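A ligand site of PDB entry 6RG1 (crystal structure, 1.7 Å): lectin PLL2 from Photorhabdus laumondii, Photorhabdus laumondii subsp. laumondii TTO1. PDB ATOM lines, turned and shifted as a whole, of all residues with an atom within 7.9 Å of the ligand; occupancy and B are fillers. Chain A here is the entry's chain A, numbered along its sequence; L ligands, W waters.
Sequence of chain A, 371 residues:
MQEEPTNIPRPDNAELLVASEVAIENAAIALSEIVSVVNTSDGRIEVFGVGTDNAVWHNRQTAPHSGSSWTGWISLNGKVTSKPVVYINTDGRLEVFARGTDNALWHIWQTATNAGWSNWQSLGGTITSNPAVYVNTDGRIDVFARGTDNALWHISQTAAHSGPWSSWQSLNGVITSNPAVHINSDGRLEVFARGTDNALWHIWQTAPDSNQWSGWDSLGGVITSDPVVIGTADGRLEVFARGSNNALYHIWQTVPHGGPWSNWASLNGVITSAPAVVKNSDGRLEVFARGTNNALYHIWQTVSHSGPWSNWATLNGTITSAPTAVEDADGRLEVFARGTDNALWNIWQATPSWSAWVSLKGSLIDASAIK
An oxygen (O2) of the ligand sits at hydrogen-bond distance from the side-chain amide nitrogen (NE2) of Gln 349.
The indole nitrogen (NE1) of Trp 354 lies within hydrogen-bond range of an oxygen (O3) of the ligand (3.0 Å).
The side-chain carboxylate (OE1) of Glu 286 sits at hydrogen-bond distance from an oxygen (O1) of the ligand (2.4 Å).
The guanidinium group of Arg 284 lies within hydrogen-bond range of an oxygen (O1) of the ligand (2.8 Å).
The side-chain amide nitrogen of Gln 349 is in hydrogen-bond range of the side-chain carboxylate of Glu 286, 3.5 Å away.
O of Trp 300 is in hydrogen-bond range of N of Ser 310 (2.7 Å).
OE2 of Glu 286 sits at hydrogen-bond distance from ND1 of His 298, at 2.6 Å.
The backbone NH (N) of Ala 313 is in hydrogen-bond range of the backbone carbonyl oxygen (O) of His 298 (2.9 Å).
The side-chain carboxylate of Asp 282 lies within salt-bridge range of the guanidinium group of Arg 284 (2.8 Å).
The side-chain amide nitrogen (ND2) of Asn 280 lies within hydrogen-bond range of the side-chain carboxylate (OE1) of Glu 286 (3.0 Å).
O of Gln 349 is in hydrogen-bond range of NH1 of Arg 332 (2.7 Å).
The guanidinium group (NH1) of Arg 284 sits at hydrogen-bond distance from the backbone carbonyl oxygen (O) of Gln 301, 2.9 Å away.
ND2 of Asn 280 touches O1 of the ligand, 3.8 Å away.
His 298 touches the ligand.
Trp 300 touches the ligand (CG to O1, 3.3 Å).
Hydrophobic or aromatic side chains within 4 Å of the ligand: His 298, Trp 300 and Trp 354.
Seven residues have an atom within 4 Å of the ligand: Asn 280, Arg 284, Glu 286, His 298, Trp 300, Gln 349 and Trp 354.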
ATOM      1  N   ASN A 280      -3.524   1.153   8.023  1.00  0.00           N
ATOM      2  CA  ASN A 280      -2.619   0.552   9.030  1.00  0.00           C
ATOM      3  C   ASN A 280      -3.368  -0.545   9.798  1.00  0.00           C
ATOM      4  O   ASN A 280      -4.618  -0.568   9.759  1.00  0.00           O
ATOM      5  CB  ASN A 280      -2.072   1.609   9.995  1.00  0.00           C
ATOM      6  CG  ASN A 280      -0.938   2.386   9.376  1.00  0.00           C
ATOM      7  OD1 ASN A 280       0.197   1.902   9.385  1.00  0.00           O
ATOM      8  ND2 ASN A 280      -1.245   3.545   8.826  1.00  0.00           N
ATOM      9  N   ASP A 282      -4.004  -0.701  12.805  1.00  0.00           N
ATOM     10  CA  ASP A 282      -4.833  -0.075  13.879  1.00  0.00           C
ATOM     11  C   ASP A 282      -5.961   0.775  13.291  1.00  0.00           C
ATOM     12  O   ASP A 282      -6.638   1.470  14.081  1.00  0.00           O
ATOM     13  CB  ASP A 282      -3.986   0.767  14.824  1.00  0.00           C
ATOM     14  CG  ASP A 282      -3.306   1.955  14.172  1.00  0.00           C
ATOM     15  OD1 ASP A 282      -3.576   2.183  12.975  1.00  0.00           O
ATOM     16  OD2 ASP A 282      -2.494   2.617  14.848  1.00  0.00           O
ATOM     17  N   ARG A 284      -5.619   3.354  11.139  1.00  0.00           N
ATOM     18  CA  ARG A 284      -5.162   4.704  10.696  1.00  0.00           C
ATOM     19  C   ARG A 284      -4.921   4.666   9.182  1.00  0.00           C
ATOM     20  O   ARG A 284      -4.151   3.816   8.726  1.00  0.00           O
ATOM     21  CB  ARG A 284      -3.894   5.137  11.438  1.00  0.00           C
ATOM     22  CG  ARG A 284      -4.128   5.517  12.891  1.00  0.00           C
ATOM     23  CD  ARG A 284      -2.833   5.829  13.641  1.00  0.00           C
ATOM     24  NE  ARG A 284      -1.772   4.872  13.354  1.00  0.00           N
ATOM     25  CZ  ARG A 284      -0.776   5.034  12.485  1.00  0.00           C
ATOM     26  NH1 ARG A 284      -0.665   6.142  11.772  1.00  0.00           N
ATOM     27  NH2 ARG A 284       0.109   4.071  12.325  1.00  0.00           N
ATOM     28  N   LEU A 285      -5.562   5.556   8.437  1.00  0.00           N
ATOM     29  CA  LEU A 285      -5.323   5.679   6.976  1.00  0.00           C
ATOM     30  C   LEU A 285      -3.932   6.280   6.756  1.00  0.00           C
ATOM     31  O   LEU A 285      -3.451   7.056   7.616  1.00  0.00           O
ATOM     32  CB  LEU A 285      -6.408   6.510   6.301  1.00  0.00           C
ATOM     33  CG  LEU A 285      -7.817   5.932   6.352  1.00  0.00           C
ATOM     34  CD1 LEU A 285      -8.775   6.804   5.565  1.00  0.00           C
ATOM     35  CD2 LEU A 285      -7.847   4.500   5.837  1.00  0.00           C
ATOM     36  N   GLU A 286      -3.311   5.906   5.651  1.00  0.00           N
ATOM     37  CA  GLU A 286      -1.988   6.417   5.251  1.00  0.00           C
ATOM     38  C   GLU A 286      -1.967   6.487   3.726  1.00  0.00           C
ATOM     39  O   GLU A 286      -2.479   5.552   3.074  1.00  0.00           O
ATOM     40  CB  GLU A 286      -0.898   5.543   5.850  1.00  0.00           C
ATOM     41  CG  GLU A 286       0.506   6.097   5.685  1.00  0.00           C
ATOM     42  CD  GLU A 286       1.501   5.626   6.728  1.00  0.00           C
ATOM     43  OE1 GLU A 286       1.074   5.008   7.735  1.00  0.00           O
ATOM     44  OE2 GLU A 286       2.710   5.881   6.536  1.00  0.00           O
ATOM     45  N   VAL A 287      -1.425   7.581   3.187  1.00  0.00           N
ATOM     46  CA  VAL A 287      -1.362   7.832   1.716  1.00  0.00           C
ATOM     47  C   VAL A 287       0.102   7.999   1.325  1.00  0.00           C
ATOM     48  O   VAL A 287       0.869   8.630   2.077  1.00  0.00           O
ATOM     49  CB  VAL A 287      -2.235   9.030   1.305  1.00  0.00           C
ATOM     50  CG1 VAL A 287      -2.192   9.258  -0.194  1.00  0.00           C
ATOM     51  CG2 VAL A 287      -3.679   8.847   1.770  1.00  0.00           C
ATOM     52  N   PHE A 288       0.462   7.406   0.194  1.00  0.00           N
ATOM     53  CA  PHE A 288       1.816   7.432  -0.409  1.00  0.00           C
ATOM     54  C   PHE A 288       1.697   8.091  -1.784  1.00  0.00           C
ATOM     55  O   PHE A 288       0.709   7.829  -2.504  1.00  0.00           O
ATOM     56  CB  PHE A 288       2.371   6.016  -0.473  1.00  0.00           C
ATOM     57  CG  PHE A 288       2.550   5.383   0.881  1.00  0.00           C
ATOM     58  CD1 PHE A 288       1.495   4.715   1.496  1.00  0.00           C
ATOM     59  CD2 PHE A 288       3.753   5.495   1.564  1.00  0.00           C
ATOM     60  CE1 PHE A 288       1.654   4.156   2.750  1.00  0.00           C
ATOM     61  CE2 PHE A 288       3.911   4.936   2.818  1.00  0.00           C
ATOM     62  CZ  PHE A 288       2.865   4.260   3.411  1.00  0.00           C
ATOM     63  N   HIS A 298       4.776  10.336   2.269  1.00  0.00           N
ATOM     64  CA  HIS A 298       3.576   9.760   2.900  1.00  0.00           C
ATOM     65  C   HIS A 298       3.028  10.723   3.938  1.00  0.00           C
ATOM     66  O   HIS A 298       3.747  11.637   4.411  1.00  0.00           O
ATOM     67  CB  HIS A 298       3.831   8.344   3.448  1.00  0.00           C
ATOM     68  CG  HIS A 298       4.788   8.293   4.579  1.00  0.00           C
ATOM     69  ND1 HIS A 298       4.582   7.481   5.680  1.00  0.00           N
ATOM     70  CD2 HIS A 298       5.962   8.926   4.798  1.00  0.00           C
ATOM     71  CE1 HIS A 298       5.593   7.617   6.519  1.00  0.00           C
ATOM     72  NE2 HIS A 298       6.453   8.497   6.009  1.00  0.00           N
ATOM     73  N   ILE A 299       1.760  10.509   4.253  1.00  0.00           N
ATOM     74  CA  ILE A 299       0.962  11.326   5.197  1.00  0.00           C
ATOM     75  C   ILE A 299      -0.034  10.350   5.803  1.00  0.00           C
ATOM     76  O   ILE A 299      -0.487   9.439   5.082  1.00  0.00           O
ATOM     77  CB  ILE A 299       0.320  12.500   4.445  1.00  0.00           C
ATOM     78  CG1 ILE A 299      -0.366  13.496   5.379  1.00  0.00           C
ATOM     79  CG2 ILE A 299      -0.627  12.006   3.353  1.00  0.00           C
ATOM     80  CD1 ILE A 299      -0.687  14.810   4.711  1.00  0.00           C
ATOM     81  N   TRP A 300      -0.317  10.484   7.089  1.00  0.00           N
ATOM     82  CA  TRP A 300      -1.108   9.465   7.830  1.00  0.00           C
ATOM     83  C   TRP A 300      -1.982  10.136   8.870  1.00  0.00           C
ATOM     84  O   TRP A 300      -1.604  11.201   9.375  1.00  0.00           O
ATOM     85  CB  TRP A 300      -0.182   8.431   8.468  1.00  0.00           C
ATOM     86  CG  TRP A 300       0.852   9.030   9.377  1.00  0.00           C
ATOM     87  CD1 TRP A 300       0.757   9.194  10.727  1.00  0.00           C
ATOM     88  CD2 TRP A 300       2.125   9.551   8.994  1.00  0.00           C
ATOM     89  NE1 TRP A 300       1.902   9.775  11.209  1.00  0.00           N
ATOM     90  CE2 TRP A 300       2.755  10.012  10.176  1.00  0.00           C
ATOM     91  CE3 TRP A 300       2.811   9.681   7.775  1.00  0.00           C
ATOM     92  CZ2 TRP A 300       4.025  10.577  10.161  1.00  0.00           C
ATOM     93  CZ3 TRP A 300       4.058  10.245   7.771  1.00  0.00           C
ATOM     94  CH2 TRP A 300       4.666  10.685   8.942  1.00  0.00           C
ATOM     95  N   GLN A 301      -3.106   9.498   9.183  1.00  0.00           N
ATOM     96  CA  GLN A 301      -3.877   9.813  10.406  1.00  0.00           C
ATOM     97  C   GLN A 301      -2.993   9.519  11.619  1.00  0.00           C
ATOM     98  O   GLN A 301      -2.335   8.484  11.625  1.00  0.00           O
ATOM     99  CB  GLN A 301      -5.159   8.984  10.446  1.00  0.00           C
ATOM    100  CG  GLN A 301      -6.134   9.360   9.349  1.00  0.00           C
ATOM    101  CD  GLN A 301      -7.418   8.606   9.542  1.00  0.00           C
ATOM    102  OE1 GLN A 301      -7.468   7.390   9.385  1.00  0.00           O
ATOM    103  NE2 GLN A 301      -8.463   9.311   9.930  1.00  0.00           N
ATOM    104  N   THR A 302      -2.984  10.421  12.596  1.00  0.00           N
ATOM    105  CA  THR A 302      -2.247  10.267  13.875  1.00  0.00           C
ATOM    106  C   THR A 302      -3.226   9.802  14.954  1.00  0.00           C
ATOM    107  O   THR A 302      -4.419  10.074  14.813  1.00  0.00           O
ATOM    108  CB  THR A 302      -1.544  11.582  14.272  1.00  0.00           C
ATOM    109  OG1 THR A 302      -2.534  12.539  14.629  1.00  0.00           O
ATOM    110  CG2 THR A 302      -0.685  12.135  13.165  1.00  0.00           C
ATOM    111  N   SER A 310      -1.371  13.821   9.836  1.00  0.00           N
ATOM    112  CA  SER A 310       0.023  14.312   9.954  1.00  0.00           C
ATOM    113  C   SER A 310       0.293  15.338   8.857  1.00  0.00           C
ATOM    114  O   SER A 310      -0.586  15.592   8.014  1.00  0.00           O
ATOM    115  CB  SER A 310       0.991  13.158   9.840  1.00  0.00           C
ATOM    116  OG  SER A 310       1.107  12.747   8.481  1.00  0.00           O
ATOM    117  N   ALA A 313       5.774  13.609   5.107  1.00  0.00           N
ATOM    118  CA  ALA A 313       7.171  13.247   5.436  1.00  0.00           C
ATOM    119  C   ALA A 313       7.750  12.458   4.265  1.00  0.00           C
ATOM    120  O   ALA A 313       7.004  11.709   3.595  1.00  0.00           O
ATOM    121  CB  ALA A 313       7.241  12.468   6.720  1.00  0.00           C
ATOM    122  N   THR A 314       9.038  12.628   4.010  1.00  0.00           N
ATOM    123  CA  THR A 314       9.733  11.946   2.898  1.00  0.00           C
ATOM    124  C   THR A 314      10.160  10.550   3.364  1.00  0.00           C
ATOM    125  O   THR A 314      10.463  10.386   4.561  1.00  0.00           O
ATOM    126  CB  THR A 314      10.917  12.765   2.377  1.00  0.00           C
ATOM    127  OG1 THR A 314      11.363  12.108   1.193  1.00  0.00           O
ATOM    128  CG2 THR A 314      12.048  12.893   3.374  1.00  0.00           C
ATOM    129  N   LEU A 315      10.187   9.602   2.432  1.00  0.00           N
ATOM    130  CA  LEU A 315      10.832   8.281   2.602  1.00  0.00           C
ATOM    131  C   LEU A 315      11.994   8.173   1.604  1.00  0.00           C
ATOM    132  O   LEU A 315      12.536   7.066   1.441  1.00  0.00           O
ATOM    133  CB  LEU A 315       9.784   7.185   2.396  1.00  0.00           C
ATOM    134  CG  LEU A 315       8.771   7.067   3.544  1.00  0.00           C
ATOM    135  CD1 LEU A 315       7.634   6.121   3.174  1.00  0.00           C
ATOM    136  CD2 LEU A 315       9.453   6.598   4.817  1.00  0.00           C
ATOM    137  N   ARG A 332       2.680  -4.434   9.411  1.00  0.00           N
ATOM    138  CA  ARG A 332       3.524  -3.318   8.930  1.00  0.00           C
ATOM    139  C   ARG A 332       3.155  -3.002   7.471  1.00  0.00           C
ATOM    140  O   ARG A 332       2.962  -3.952   6.679  1.00  0.00           O
ATOM    141  CB  ARG A 332       5.009  -3.648   9.028  1.00  0.00           C
ATOM    142  CG  ARG A 332       5.486  -4.016  10.433  1.00  0.00           C
ATOM    143  CD  ARG A 332       5.209  -2.939  11.460  1.00  0.00           C
ATOM    144  NE  ARG A 332       5.751  -3.326  12.768  1.00  0.00           N
ATOM    145  CZ  ARG A 332       6.960  -2.988  13.237  1.00  0.00           C
ATOM    146  NH1 ARG A 332       7.780  -2.227  12.536  1.00  0.00           N
ATOM    147  NH2 ARG A 332       7.339  -3.420  14.427  1.00  0.00           N
ATOM    148  N   LEU A 333       3.070  -1.717   7.149  1.00  0.00           N
ATOM    149  CA  LEU A 333       2.891  -1.252   5.750  1.00  0.00           C
ATOM    150  C   LEU A 333       4.147  -1.588   4.951  1.00  0.00           C
ATOM    151  O   LEU A 333       5.277  -1.415   5.467  1.00  0.00           O
ATOM    152  CB  LEU A 333       2.599   0.252   5.730  1.00  0.00           C
ATOM    153  CG  LEU A 333       1.299   0.691   6.381  1.00  0.00           C
ATOM    154  CD1 LEU A 333       1.030   2.156   6.088  1.00  0.00           C
ATOM    155  CD2 LEU A 333       0.119  -0.154   5.935  1.00  0.00           C
ATOM    156  N   TRP A 348       9.537  -0.642   4.003  1.00  0.00           N
ATOM    157  CA  TRP A 348       8.492  -1.091   4.957  1.00  0.00           C
ATOM    158  C   TRP A 348       8.640  -0.381   6.295  1.00  0.00           C
ATOM    159  O   TRP A 348       9.714   0.164   6.595  1.00  0.00           O
ATOM    160  CB  TRP A 348       8.468  -2.611   5.069  1.00  0.00           C
ATOM    161  CG  TRP A 348       9.715  -3.248   5.595  1.00  0.00           C
ATOM    162  CD1 TRP A 348      10.791  -3.701   4.891  1.00  0.00           C
ATOM    163  CD2 TRP A 348       9.977  -3.566   6.974  1.00  0.00           C
ATOM    164  NE1 TRP A 348      11.707  -4.264   5.736  1.00  0.00           N
ATOM    165  CE2 TRP A 348      11.242  -4.187   7.020  1.00  0.00           C
ATOM    166  CE3 TRP A 348       9.271  -3.383   8.170  1.00  0.00           C
ATOM    167  CZ2 TRP A 348      11.812  -4.629   8.215  1.00  0.00           C
ATOM    168  CZ3 TRP A 348       9.829  -3.809   9.350  1.00  0.00           C
ATOM    169  CH2 TRP A 348      11.089  -4.421   9.376  1.00  0.00           C
ATOM    170  N   GLN A 349       7.554  -0.413   7.068  1.00  0.00           N
ATOM    171  CA  GLN A 349       7.292   0.444   8.245  1.00  0.00           C
ATOM    172  C   GLN A 349       7.982  -0.171   9.481  1.00  0.00           C
ATOM    173  O   GLN A 349       7.275  -0.750  10.307  1.00  0.00           O
ATOM    174  CB  GLN A 349       5.766   0.525   8.331  1.00  0.00           C
ATOM    175  CG  GLN A 349       5.194   1.558   9.292  1.00  0.00           C
ATOM    176  CD  GLN A 349       3.698   1.402   9.351  1.00  0.00           C
ATOM    177  OE1 GLN A 349       3.175   0.290   9.450  1.00  0.00           O
ATOM    178  NE2 GLN A 349       2.987   2.517   9.276  1.00  0.00           N
ATOM    179  N   ALA A 350       9.318  -0.063   9.579  1.00  0.00           N
ATOM    180  CA  ALA A 350      10.160  -0.678  10.635  1.00  0.00           C
ATOM    181  C   ALA A 350      10.269   0.254  11.851  1.00  0.00           C
ATOM    182  O   ALA A 350       9.678   1.340  11.778  1.00  0.00           O
ATOM    183  CB  ALA A 350      11.536  -1.006  10.086  1.00  0.00           C
ATOM    184  N   TRP A 354      11.369   3.939   9.223  1.00  0.00           N
ATOM    185  CA  TRP A 354      11.123   2.941   8.134  1.00  0.00           C
ATOM    186  C   TRP A 354      12.430   2.245   7.755  1.00  0.00           C
ATOM    187  O   TRP A 354      13.524   2.769   8.065  1.00  0.00           O
ATOM    188  CB  TRP A 354      10.476   3.577   6.898  1.00  0.00           C
ATOM    189  CG  TRP A 354       8.999   3.808   7.020  1.00  0.00           C
ATOM    190  CD1 TRP A 354       8.352   4.540   7.971  1.00  0.00           C
ATOM    191  CD2 TRP A 354       7.976   3.316   6.138  1.00  0.00           C
ATOM    192  NE1 TRP A 354       7.006   4.523   7.748  1.00  0.00           N
ATOM    193  CE2 TRP A 354       6.742   3.783   6.638  1.00  0.00           C
ATOM    194  CE3 TRP A 354       7.977   2.520   4.982  1.00  0.00           C
ATOM    195  CZ2 TRP A 354       5.522   3.482   6.016  1.00  0.00           C
ATOM    196  CZ3 TRP A 354       6.776   2.216   4.374  1.00  0.00           C
ATOM    197  CH2 TRP A 354       5.570   2.690   4.887  1.00  0.00           C
HETATM  198  C1  LIG L   1       2.750   6.028  10.651  1.00  0.00           C
HETATM  199  C2  LIG L   1       3.890   6.290   9.692  1.00  0.00           C
HETATM  200  C3  LIG L   1       5.174   6.484  10.476  1.00  0.00           C
HETATM  201  C4  LIG L   1       5.441   5.259  11.331  1.00  0.00           C
HETATM  202  C5  LIG L   1       4.249   5.029  12.258  1.00  0.00           C
HETATM  203  C6  LIG L   1       4.374   3.769  13.083  1.00  0.00           C
HETATM  204  O1  LIG L   1       1.532   5.817   9.993  1.00  0.00           O
HETATM  205  O2  LIG L   1       4.004   5.229   8.743  1.00  0.00           O
HETATM  206  O3  LIG L   1       6.263   6.728   9.591  1.00  0.00           O
HETATM  207  O4  LIG L   1       6.631   5.420  12.094  1.00  0.00           O
HETATM  208  O5  LIG L   1       3.040   4.886  11.467  1.00  0.00           O
HETATM  209  O   HOH W   1       6.618   6.560  14.451  1.00  0.00           O
HETATM  210  O   HOH W   2       8.333   8.236  10.638  1.00  0.00           O
